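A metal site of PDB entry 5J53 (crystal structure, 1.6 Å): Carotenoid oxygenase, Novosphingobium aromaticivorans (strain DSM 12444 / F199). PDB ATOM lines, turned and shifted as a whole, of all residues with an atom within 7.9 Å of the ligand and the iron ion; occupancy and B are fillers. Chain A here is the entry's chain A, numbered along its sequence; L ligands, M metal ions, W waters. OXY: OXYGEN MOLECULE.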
ATOM      1  N   PHE A  59     -23.037   9.805  11.435  1.00  0.00           N
ATOM      2  CA  PHE A  59     -21.797   9.058  11.333  1.00  0.00           C
ATOM      3  C   PHE A  59     -21.973   7.781  10.501  1.00  0.00           C
ATOM      4  O   PHE A  59     -20.966   7.131  10.237  1.00  0.00           O
ATOM      5  CB  PHE A  59     -21.256   8.702  12.736  1.00  0.00           C
ATOM      6  CG  PHE A  59     -20.480   9.818  13.449  1.00  0.00           C
ATOM      7  CD1 PHE A  59     -20.381  11.096  12.906  1.00  0.00           C
ATOM      8  CD2 PHE A  59     -19.864   9.570  14.678  1.00  0.00           C
ATOM      9  CE1 PHE A  59     -19.675  12.108  13.569  1.00  0.00           C
ATOM     10  CE2 PHE A  59     -19.164  10.584  15.369  1.00  0.00           C
ATOM     11  CZ  PHE A  59     -19.065  11.849  14.805  1.00  0.00           C
ATOM     12  N   ASN A 120     -16.160   6.549   5.437  1.00  0.00           N
ATOM     13  CA  ASN A 120     -16.788   7.853   5.446  1.00  0.00           C
ATOM     14  C   ASN A 120     -16.109   8.874   6.349  1.00  0.00           C
ATOM     15  O   ASN A 120     -16.651   9.974   6.516  1.00  0.00           O
ATOM     16  CB  ASN A 120     -18.271   7.731   5.828  1.00  0.00           C
ATOM     17  CG  ASN A 120     -18.482   7.463   7.320  1.00  0.00           C
ATOM     18  OD1 ASN A 120     -17.517   7.309   8.094  1.00  0.00           O
ATOM     19  ND2 ASN A 120     -19.747   7.406   7.730  1.00  0.00           N
ATOM     20  N   THR A 121     -14.952   8.554   6.938  1.00  0.00           N
ATOM     21  CA  THR A 121     -14.377   9.414   7.963  1.00  0.00           C
ATOM     22  C   THR A 121     -13.184  10.242   7.503  1.00  0.00           C
ATOM     23  O   THR A 121     -12.982  11.361   8.019  1.00  0.00           O
ATOM     24  CB  THR A 121     -13.961   8.568   9.182  1.00  0.00           C
ATOM     25  OG1 THR A 121     -15.133   7.881   9.694  1.00  0.00           O
ATOM     26  CG2 THR A 121     -13.428   9.436  10.299  1.00  0.00           C
ATOM     27  N   ASN A 122     -12.364   9.739   6.597  1.00  0.00           N
ATOM     28  CA  ASN A 122     -11.212  10.493   6.098  1.00  0.00           C
ATOM     29  C   ASN A 122     -10.994  10.188   4.624  1.00  0.00           C
ATOM     30  O   ASN A 122     -11.244   9.062   4.143  1.00  0.00           O
ATOM     31  CB  ASN A 122      -9.932  10.182   6.882  1.00  0.00           C
ATOM     32  CG  ASN A 122      -8.923  11.325   6.893  1.00  0.00           C
ATOM     33  OD1 ASN A 122      -8.940  12.221   6.024  1.00  0.00           O
ATOM     34  ND2 ASN A 122      -8.052  11.323   7.899  1.00  0.00           N
ATOM     35  N   LYS A 134     -12.315   4.334   7.421  1.00  0.00           N
ATOM     36  CA  LYS A 134     -13.310   4.130   8.473  1.00  0.00           C
ATOM     37  C   LYS A 134     -12.746   3.094   9.429  1.00  0.00           C
ATOM     38  O   LYS A 134     -12.356   2.005   9.003  1.00  0.00           O
ATOM     39  CB  LYS A 134     -14.670   3.687   7.898  1.00  0.00           C
ATOM     40  CG  LYS A 134     -15.764   3.445   8.978  1.00  0.00           C
ATOM     41  CD  LYS A 134     -16.190   4.705   9.645  1.00  0.00           C
ATOM     42  CE  LYS A 134     -17.043   4.465  10.890  1.00  0.00           C
ATOM     43  NZ  LYS A 134     -16.997   5.653  11.863  1.00  0.00           N
ATOM     44  N   GLU A 135     -12.680   3.442  10.720  1.00  0.00           N
ATOM     45  CA  GLU A 135     -11.821   2.760  11.691  1.00  0.00           C
ATOM     46  C   GLU A 135     -12.283   1.367  12.104  1.00  0.00           C
ATOM     47  O   GLU A 135     -11.636   0.791  12.987  1.00  0.00           O
ATOM     48  CB  GLU A 135     -11.695   3.640  12.929  1.00  0.00           C
ATOM     49  CG  GLU A 135     -12.991   3.756  13.703  1.00  0.00           C
ATOM     50  CD  GLU A 135     -13.005   4.983  14.584  1.00  0.00           C
ATOM     51  OE1 GLU A 135     -12.561   6.049  14.102  1.00  0.00           O
ATOM     52  OE2 GLU A 135     -13.478   4.861  15.731  1.00  0.00           O
ATOM     53  N   ALA A 166      -8.752   5.773  10.853  1.00  0.00           N
ATOM     54  CA  ALA A 166      -9.090   6.858   9.949  1.00  0.00           C
ATOM     55  C   ALA A 166      -8.343   8.134  10.293  1.00  0.00           C
ATOM     56  O   ALA A 166      -8.632   9.187   9.702  1.00  0.00           O
ATOM     57  CB  ALA A 166     -10.613   7.100   9.954  1.00  0.00           C
ATOM     58  N   HIS A 167      -7.338   8.059  11.184  1.00  0.00           N
ATOM     59  CA  HIS A 167      -6.506   9.220  11.537  1.00  0.00           C
ATOM     60  C   HIS A 167      -5.025   8.895  11.349  1.00  0.00           C
ATOM     61  O   HIS A 167      -4.210   9.053  12.270  1.00  0.00           O
ATOM     62  CB  HIS A 167      -6.818   9.683  12.947  1.00  0.00           C
ATOM     63  CG  HIS A 167      -7.943  10.665  13.025  1.00  0.00           C
ATOM     64  ND1 HIS A 167      -7.794  11.992  12.675  1.00  0.00           N
ATOM     65  CD2 HIS A 167      -9.241  10.520  13.384  1.00  0.00           C
ATOM     66  CE1 HIS A 167      -8.953  12.626  12.812  1.00  0.00           C
ATOM     67  NE2 HIS A 167      -9.847  11.750  13.236  1.00  0.00           N
ATOM     68  N   MET A 216     -13.558   3.857  22.127  1.00  0.00           N
ATOM     69  CA  MET A 216     -13.350   4.442  20.815  1.00  0.00           C
ATOM     70  C   MET A 216     -11.954   5.039  20.759  1.00  0.00           C
ATOM     71  O   MET A 216     -11.688   6.105  21.319  1.00  0.00           O
ATOM     72  CB  MET A 216     -14.371   5.513  20.509  1.00  0.00           C
ATOM     73  CG  MET A 216     -14.317   5.990  19.083  1.00  0.00           C
ATOM     74  SD  MET A 216     -15.226   7.500  18.768  1.00  0.00           S
ATOM     75  CE  MET A 216     -16.858   7.133  19.377  1.00  0.00           C
ATOM     76  N   HIS A 218     -10.263   6.621  18.351  1.00  0.00           N
ATOM     77  CA  HIS A 218     -10.492   7.315  17.097  1.00  0.00           C
ATOM     78  C   HIS A 218      -9.219   7.991  16.596  1.00  0.00           C
ATOM     79  O   HIS A 218      -8.971   8.030  15.385  1.00  0.00           O
ATOM     80  CB  HIS A 218     -11.615   8.352  17.336  1.00  0.00           C
ATOM     81  CG  HIS A 218     -11.930   9.183  16.151  1.00  0.00           C
ATOM     82  ND1 HIS A 218     -12.487   8.656  14.999  1.00  0.00           N
ATOM     83  CD2 HIS A 218     -11.830  10.520  15.936  1.00  0.00           C
ATOM     84  CE1 HIS A 218     -12.681   9.624  14.122  1.00  0.00           C
ATOM     85  NE2 HIS A 218     -12.285  10.769  14.671  1.00  0.00           N
ATOM     86  N   ASP A 219      -8.414   8.542  17.489  1.00  0.00           N
ATOM     87  CA  ASP A 219      -7.241   9.329  17.107  1.00  0.00           C
ATOM     88  C   ASP A 219      -6.054   8.920  17.988  1.00  0.00           C
ATOM     89  O   ASP A 219      -6.181   8.087  18.907  1.00  0.00           O
ATOM     90  CB  ASP A 219      -7.579  10.836  17.190  1.00  0.00           C
ATOM     91  CG  ASP A 219      -6.716  11.714  16.278  1.00  0.00           C
ATOM     92  OD1 ASP A 219      -5.731  11.252  15.637  1.00  0.00           O
ATOM     93  OD2 ASP A 219      -7.046  12.910  16.196  1.00  0.00           O
ATOM     94  N   SER A 283     -11.118  13.704  21.992  1.00  0.00           N
ATOM     95  CA  SER A 283     -11.156  12.907  20.771  1.00  0.00           C
ATOM     96  C   SER A 283      -9.954  13.236  19.892  1.00  0.00           C
ATOM     97  O   SER A 283      -9.068  12.397  19.748  1.00  0.00           O
ATOM     98  CB  SER A 283     -12.465  13.159  20.044  1.00  0.00           C
ATOM     99  OG  SER A 283     -12.526  12.415  18.830  1.00  0.00           O
ATOM    100  N   HIS A 284      -9.876  14.439  19.329  1.00  0.00           N
ATOM    101  CA  HIS A 284      -8.850  14.713  18.329  1.00  0.00           C
ATOM    102  C   HIS A 284      -7.543  15.236  18.925  1.00  0.00           C
ATOM    103  O   HIS A 284      -7.509  15.974  19.918  1.00  0.00           O
ATOM    104  CB  HIS A 284      -9.389  15.709  17.301  1.00  0.00           C
ATOM    105  CG  HIS A 284     -10.404  15.095  16.404  1.00  0.00           C
ATOM    106  ND1 HIS A 284     -11.675  15.609  16.256  1.00  0.00           N
ATOM    107  CD2 HIS A 284     -10.358  13.983  15.630  1.00  0.00           C
ATOM    108  CE1 HIS A 284     -12.368  14.836  15.427  1.00  0.00           C
ATOM    109  NE2 HIS A 284     -11.579  13.848  15.023  1.00  0.00           N
ATOM    110  N   VAL A 285      -6.465  14.864  18.229  1.00  0.00           N
ATOM    111  CA  VAL A 285      -5.098  15.218  18.566  1.00  0.00           C
ATOM    112  C   VAL A 285      -4.604  16.306  17.610  1.00  0.00           C
ATOM    113  O   VAL A 285      -4.665  16.141  16.379  1.00  0.00           O
ATOM    114  CB  VAL A 285      -4.196  13.983  18.509  1.00  0.00           C
ATOM    115  CG1 VAL A 285      -2.750  14.318  18.883  1.00  0.00           C
ATOM    116  CG2 VAL A 285      -4.783  12.911  19.454  1.00  0.00           C
ATOM    117  N   PHE A 307     -20.397  13.492  22.405  1.00  0.00           N
ATOM    118  CA  PHE A 307     -21.257  12.779  21.455  1.00  0.00           C
ATOM    119  C   PHE A 307     -22.643  12.554  22.049  1.00  0.00           C
ATOM    120  O   PHE A 307     -22.862  11.545  22.725  1.00  0.00           O
ATOM    121  CB  PHE A 307     -20.656  11.422  21.107  1.00  0.00           C
ATOM    122  CG  PHE A 307     -19.262  11.467  20.512  1.00  0.00           C
ATOM    123  CD1 PHE A 307     -18.928  12.383  19.525  1.00  0.00           C
ATOM    124  CD2 PHE A 307     -18.316  10.564  20.930  1.00  0.00           C
ATOM    125  CE1 PHE A 307     -17.645  12.385  18.985  1.00  0.00           C
ATOM    126  CE2 PHE A 307     -17.046  10.567  20.395  1.00  0.00           C
ATOM    127  CZ  PHE A 307     -16.720  11.490  19.427  1.00  0.00           C
ATOM    128  N   GLU A 353     -12.271  22.589  18.223  1.00  0.00           N
ATOM    129  CA  GLU A 353     -12.163  21.183  17.854  1.00  0.00           C
ATOM    130  C   GLU A 353     -11.673  21.138  16.412  1.00  0.00           C
ATOM    131  O   GLU A 353     -11.235  22.153  15.860  1.00  0.00           O
ATOM    132  CB  GLU A 353     -13.492  20.453  18.060  1.00  0.00           C
ATOM    133  CG  GLU A 353     -13.407  19.246  19.020  1.00  0.00           C
ATOM    134  CD  GLU A 353     -12.596  18.087  18.480  1.00  0.00           C
ATOM    135  OE1 GLU A 353     -12.008  17.323  19.278  1.00  0.00           O
ATOM    136  OE2 GLU A 353     -12.546  17.898  17.249  1.00  0.00           O
ATOM    137  N   PHE A 354     -11.696  19.964  15.816  1.00  0.00           N
ATOM    138  CA  PHE A 354     -11.088  19.705  14.517  1.00  0.00           C
ATOM    139  C   PHE A 354      -9.707  20.392  14.403  1.00  0.00           C
ATOM    140  O   PHE A 354      -9.487  21.173  13.483  1.00  0.00           O
ATOM    141  CB  PHE A 354     -12.015  20.116  13.394  1.00  0.00           C
ATOM    142  CG  PHE A 354     -13.152  19.163  13.240  1.00  0.00           C
ATOM    143  CD1 PHE A 354     -13.000  18.042  12.428  1.00  0.00           C
ATOM    144  CD2 PHE A 354     -14.299  19.298  13.982  1.00  0.00           C
ATOM    145  CE1 PHE A 354     -14.049  17.115  12.301  1.00  0.00           C
ATOM    146  CE2 PHE A 354     -15.326  18.370  13.874  1.00  0.00           C
ATOM    147  CZ  PHE A 354     -15.205  17.284  13.032  1.00  0.00           C
ATOM    148  N   PRO A 355      -8.776  20.044  15.292  1.00  0.00           N
ATOM    149  CA  PRO A 355      -7.442  20.674  15.266  1.00  0.00           C
ATOM    150  C   PRO A 355      -6.578  20.235  14.090  1.00  0.00           C
ATOM    151  O   PRO A 355      -6.586  19.062  13.728  1.00  0.00           O
ATOM    152  CB  PRO A 355      -6.819  20.176  16.571  1.00  0.00           C
ATOM    153  CG  PRO A 355      -7.470  18.791  16.748  1.00  0.00           C
ATOM    154  CD  PRO A 355      -8.881  18.959  16.282  1.00  0.00           C
ATOM    155  N   GLU A 418     -13.992  21.213   8.552  1.00  0.00           N
ATOM    156  CA  GLU A 418     -12.616  21.134   9.028  1.00  0.00           C
ATOM    157  C   GLU A 418     -11.667  21.885   8.090  1.00  0.00           C
ATOM    158  O   GLU A 418     -11.676  21.637   6.873  1.00  0.00           O
ATOM    159  CB  GLU A 418     -12.183  19.675   9.160  1.00  0.00           C
ATOM    160  CG  GLU A 418     -10.707  19.485   9.604  1.00  0.00           C
ATOM    161  CD  GLU A 418     -10.200  18.056   9.409  1.00  0.00           C
ATOM    162  OE1 GLU A 418     -10.192  17.584   8.247  1.00  0.00           O
ATOM    163  OE2 GLU A 418      -9.811  17.390  10.409  1.00  0.00           O
ATOM    164  N   PHE A 473     -22.561  17.574   5.844  1.00  0.00           N
ATOM    165  CA  PHE A 473     -21.577  17.511   6.925  1.00  0.00           C
ATOM    166  C   PHE A 473     -20.378  16.673   6.499  1.00  0.00           C
ATOM    167  O   PHE A 473     -20.541  15.565   6.004  1.00  0.00           O
ATOM    168  CB  PHE A 473     -22.258  16.913   8.161  1.00  0.00           C
ATOM    169  CG  PHE A 473     -21.348  16.496   9.259  1.00  0.00           C
ATOM    170  CD1 PHE A 473     -20.797  17.430  10.117  1.00  0.00           C
ATOM    171  CD2 PHE A 473     -21.063  15.142   9.459  1.00  0.00           C
ATOM    172  CE1 PHE A 473     -19.947  17.042  11.166  1.00  0.00           C
ATOM    173  CE2 PHE A 473     -20.222  14.750  10.508  1.00  0.00           C
ATOM    174  CZ  PHE A 473     -19.668  15.699  11.350  1.00  0.00           C
ATOM    175  N   GLY A 474     -19.180  17.239   6.633  1.00  0.00           N
ATOM    176  CA  GLY A 474     -17.954  16.535   6.339  1.00  0.00           C
ATOM    177  C   GLY A 474     -17.262  16.017   7.585  1.00  0.00           C
ATOM    178  O   GLY A 474     -17.477  16.486   8.696  1.00  0.00           O
ATOM    179  N   LEU A 475     -16.382  15.030   7.392  1.00  0.00           N
ATOM    180  CA  LEU A 475     -15.468  14.652   8.453  1.00  0.00           C
ATOM    181  C   LEU A 475     -14.080  15.166   8.056  1.00  0.00           C
ATOM    182  O   LEU A 475     -13.900  16.381   8.007  1.00  0.00           O
ATOM    183  CB  LEU A 475     -15.557  13.155   8.731  1.00  0.00           C
ATOM    184  CG  LEU A 475     -16.884  12.856   9.507  1.00  0.00           C
ATOM    185  CD1 LEU A 475     -17.175  11.377   9.597  1.00  0.00           C
ATOM    186  CD2 LEU A 475     -16.786  13.407  10.927  1.00  0.00           C
ATOM    187  N   HIS A 476     -13.108  14.314   7.776  1.00  0.00           N
ATOM    188  CA  HIS A 476     -11.721  14.773   7.642  1.00  0.00           C
ATOM    189  C   HIS A 476     -11.285  14.851   6.189  1.00  0.00           C
ATOM    190  O   HIS A 476     -11.849  14.206   5.296  1.00  0.00           O
ATOM    191  CB  HIS A 476     -10.812  13.900   8.455  1.00  0.00           C
ATOM    192  CG  HIS A 476     -11.158  13.887   9.912  1.00  0.00           C
ATOM    193  ND1 HIS A 476     -10.921  14.962  10.725  1.00  0.00           N
ATOM    194  CD2 HIS A 476     -11.794  12.969  10.666  1.00  0.00           C
ATOM    195  CE1 HIS A 476     -11.338  14.679  11.958  1.00  0.00           C
ATOM    196  NE2 HIS A 476     -11.879  13.481  11.941  1.00  0.00           N
HETATM  197  O1  OXY L   1     -14.304  12.957  14.096  1.00  0.00           O
HETATM  198  O2  OXY L   1     -14.231  11.996  13.368  1.00  0.00           O
HETATM  199 FE    FE M   1     -11.809  12.403  13.632  1.00  0.00          FE
HETATM  200  O   HOH W   1     -14.584  13.042  17.151  1.00  0.00           O
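ND1 of His 476 is in hydrogen-bond range of OE2 of Glu 418, at 2.7 Å.
ND1 of His 284 sits at hydrogen-bond distance from OE2 of Glu 353.
A ring nitrogen (ND1) of His 218 is in hydrogen-bond range of the side-chain carboxylate (OE1) of Glu 135.
The backbone carbonyl oxygen (O) of Thr 121 lies within hydrogen-bond range of the backbone NH (N) of His 476 (3.0 Å).
CD2 of Leu 475 touches O2 of the ligand, 3.8 Å away.
Hydrophobic or aromatic side chains that line the ligand: His 218, His 284, Leu 475 and His 476.
Within 4 Å of the ligand: His 218, His 284, Leu 475 and His 476.
Within 4 Å of the iron ion: His 167, His 218, His 284 and His 476.
The nearest printed residue that does not touch the iron ion is Thr 121 (4.7 Å).
The iron ion is bound by a ring nitrogen (NE2) of His 218 (2.0 Å), a ring nitrogen (NE2) of His 476 (2.0 Å), a ring nitrogen (NE2) of His 284 (2.0 Å), a ring nitrogen (NE2) of His 167 (2.1 Å) and an oxygen (O2) of the ligand (2.5 Å).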
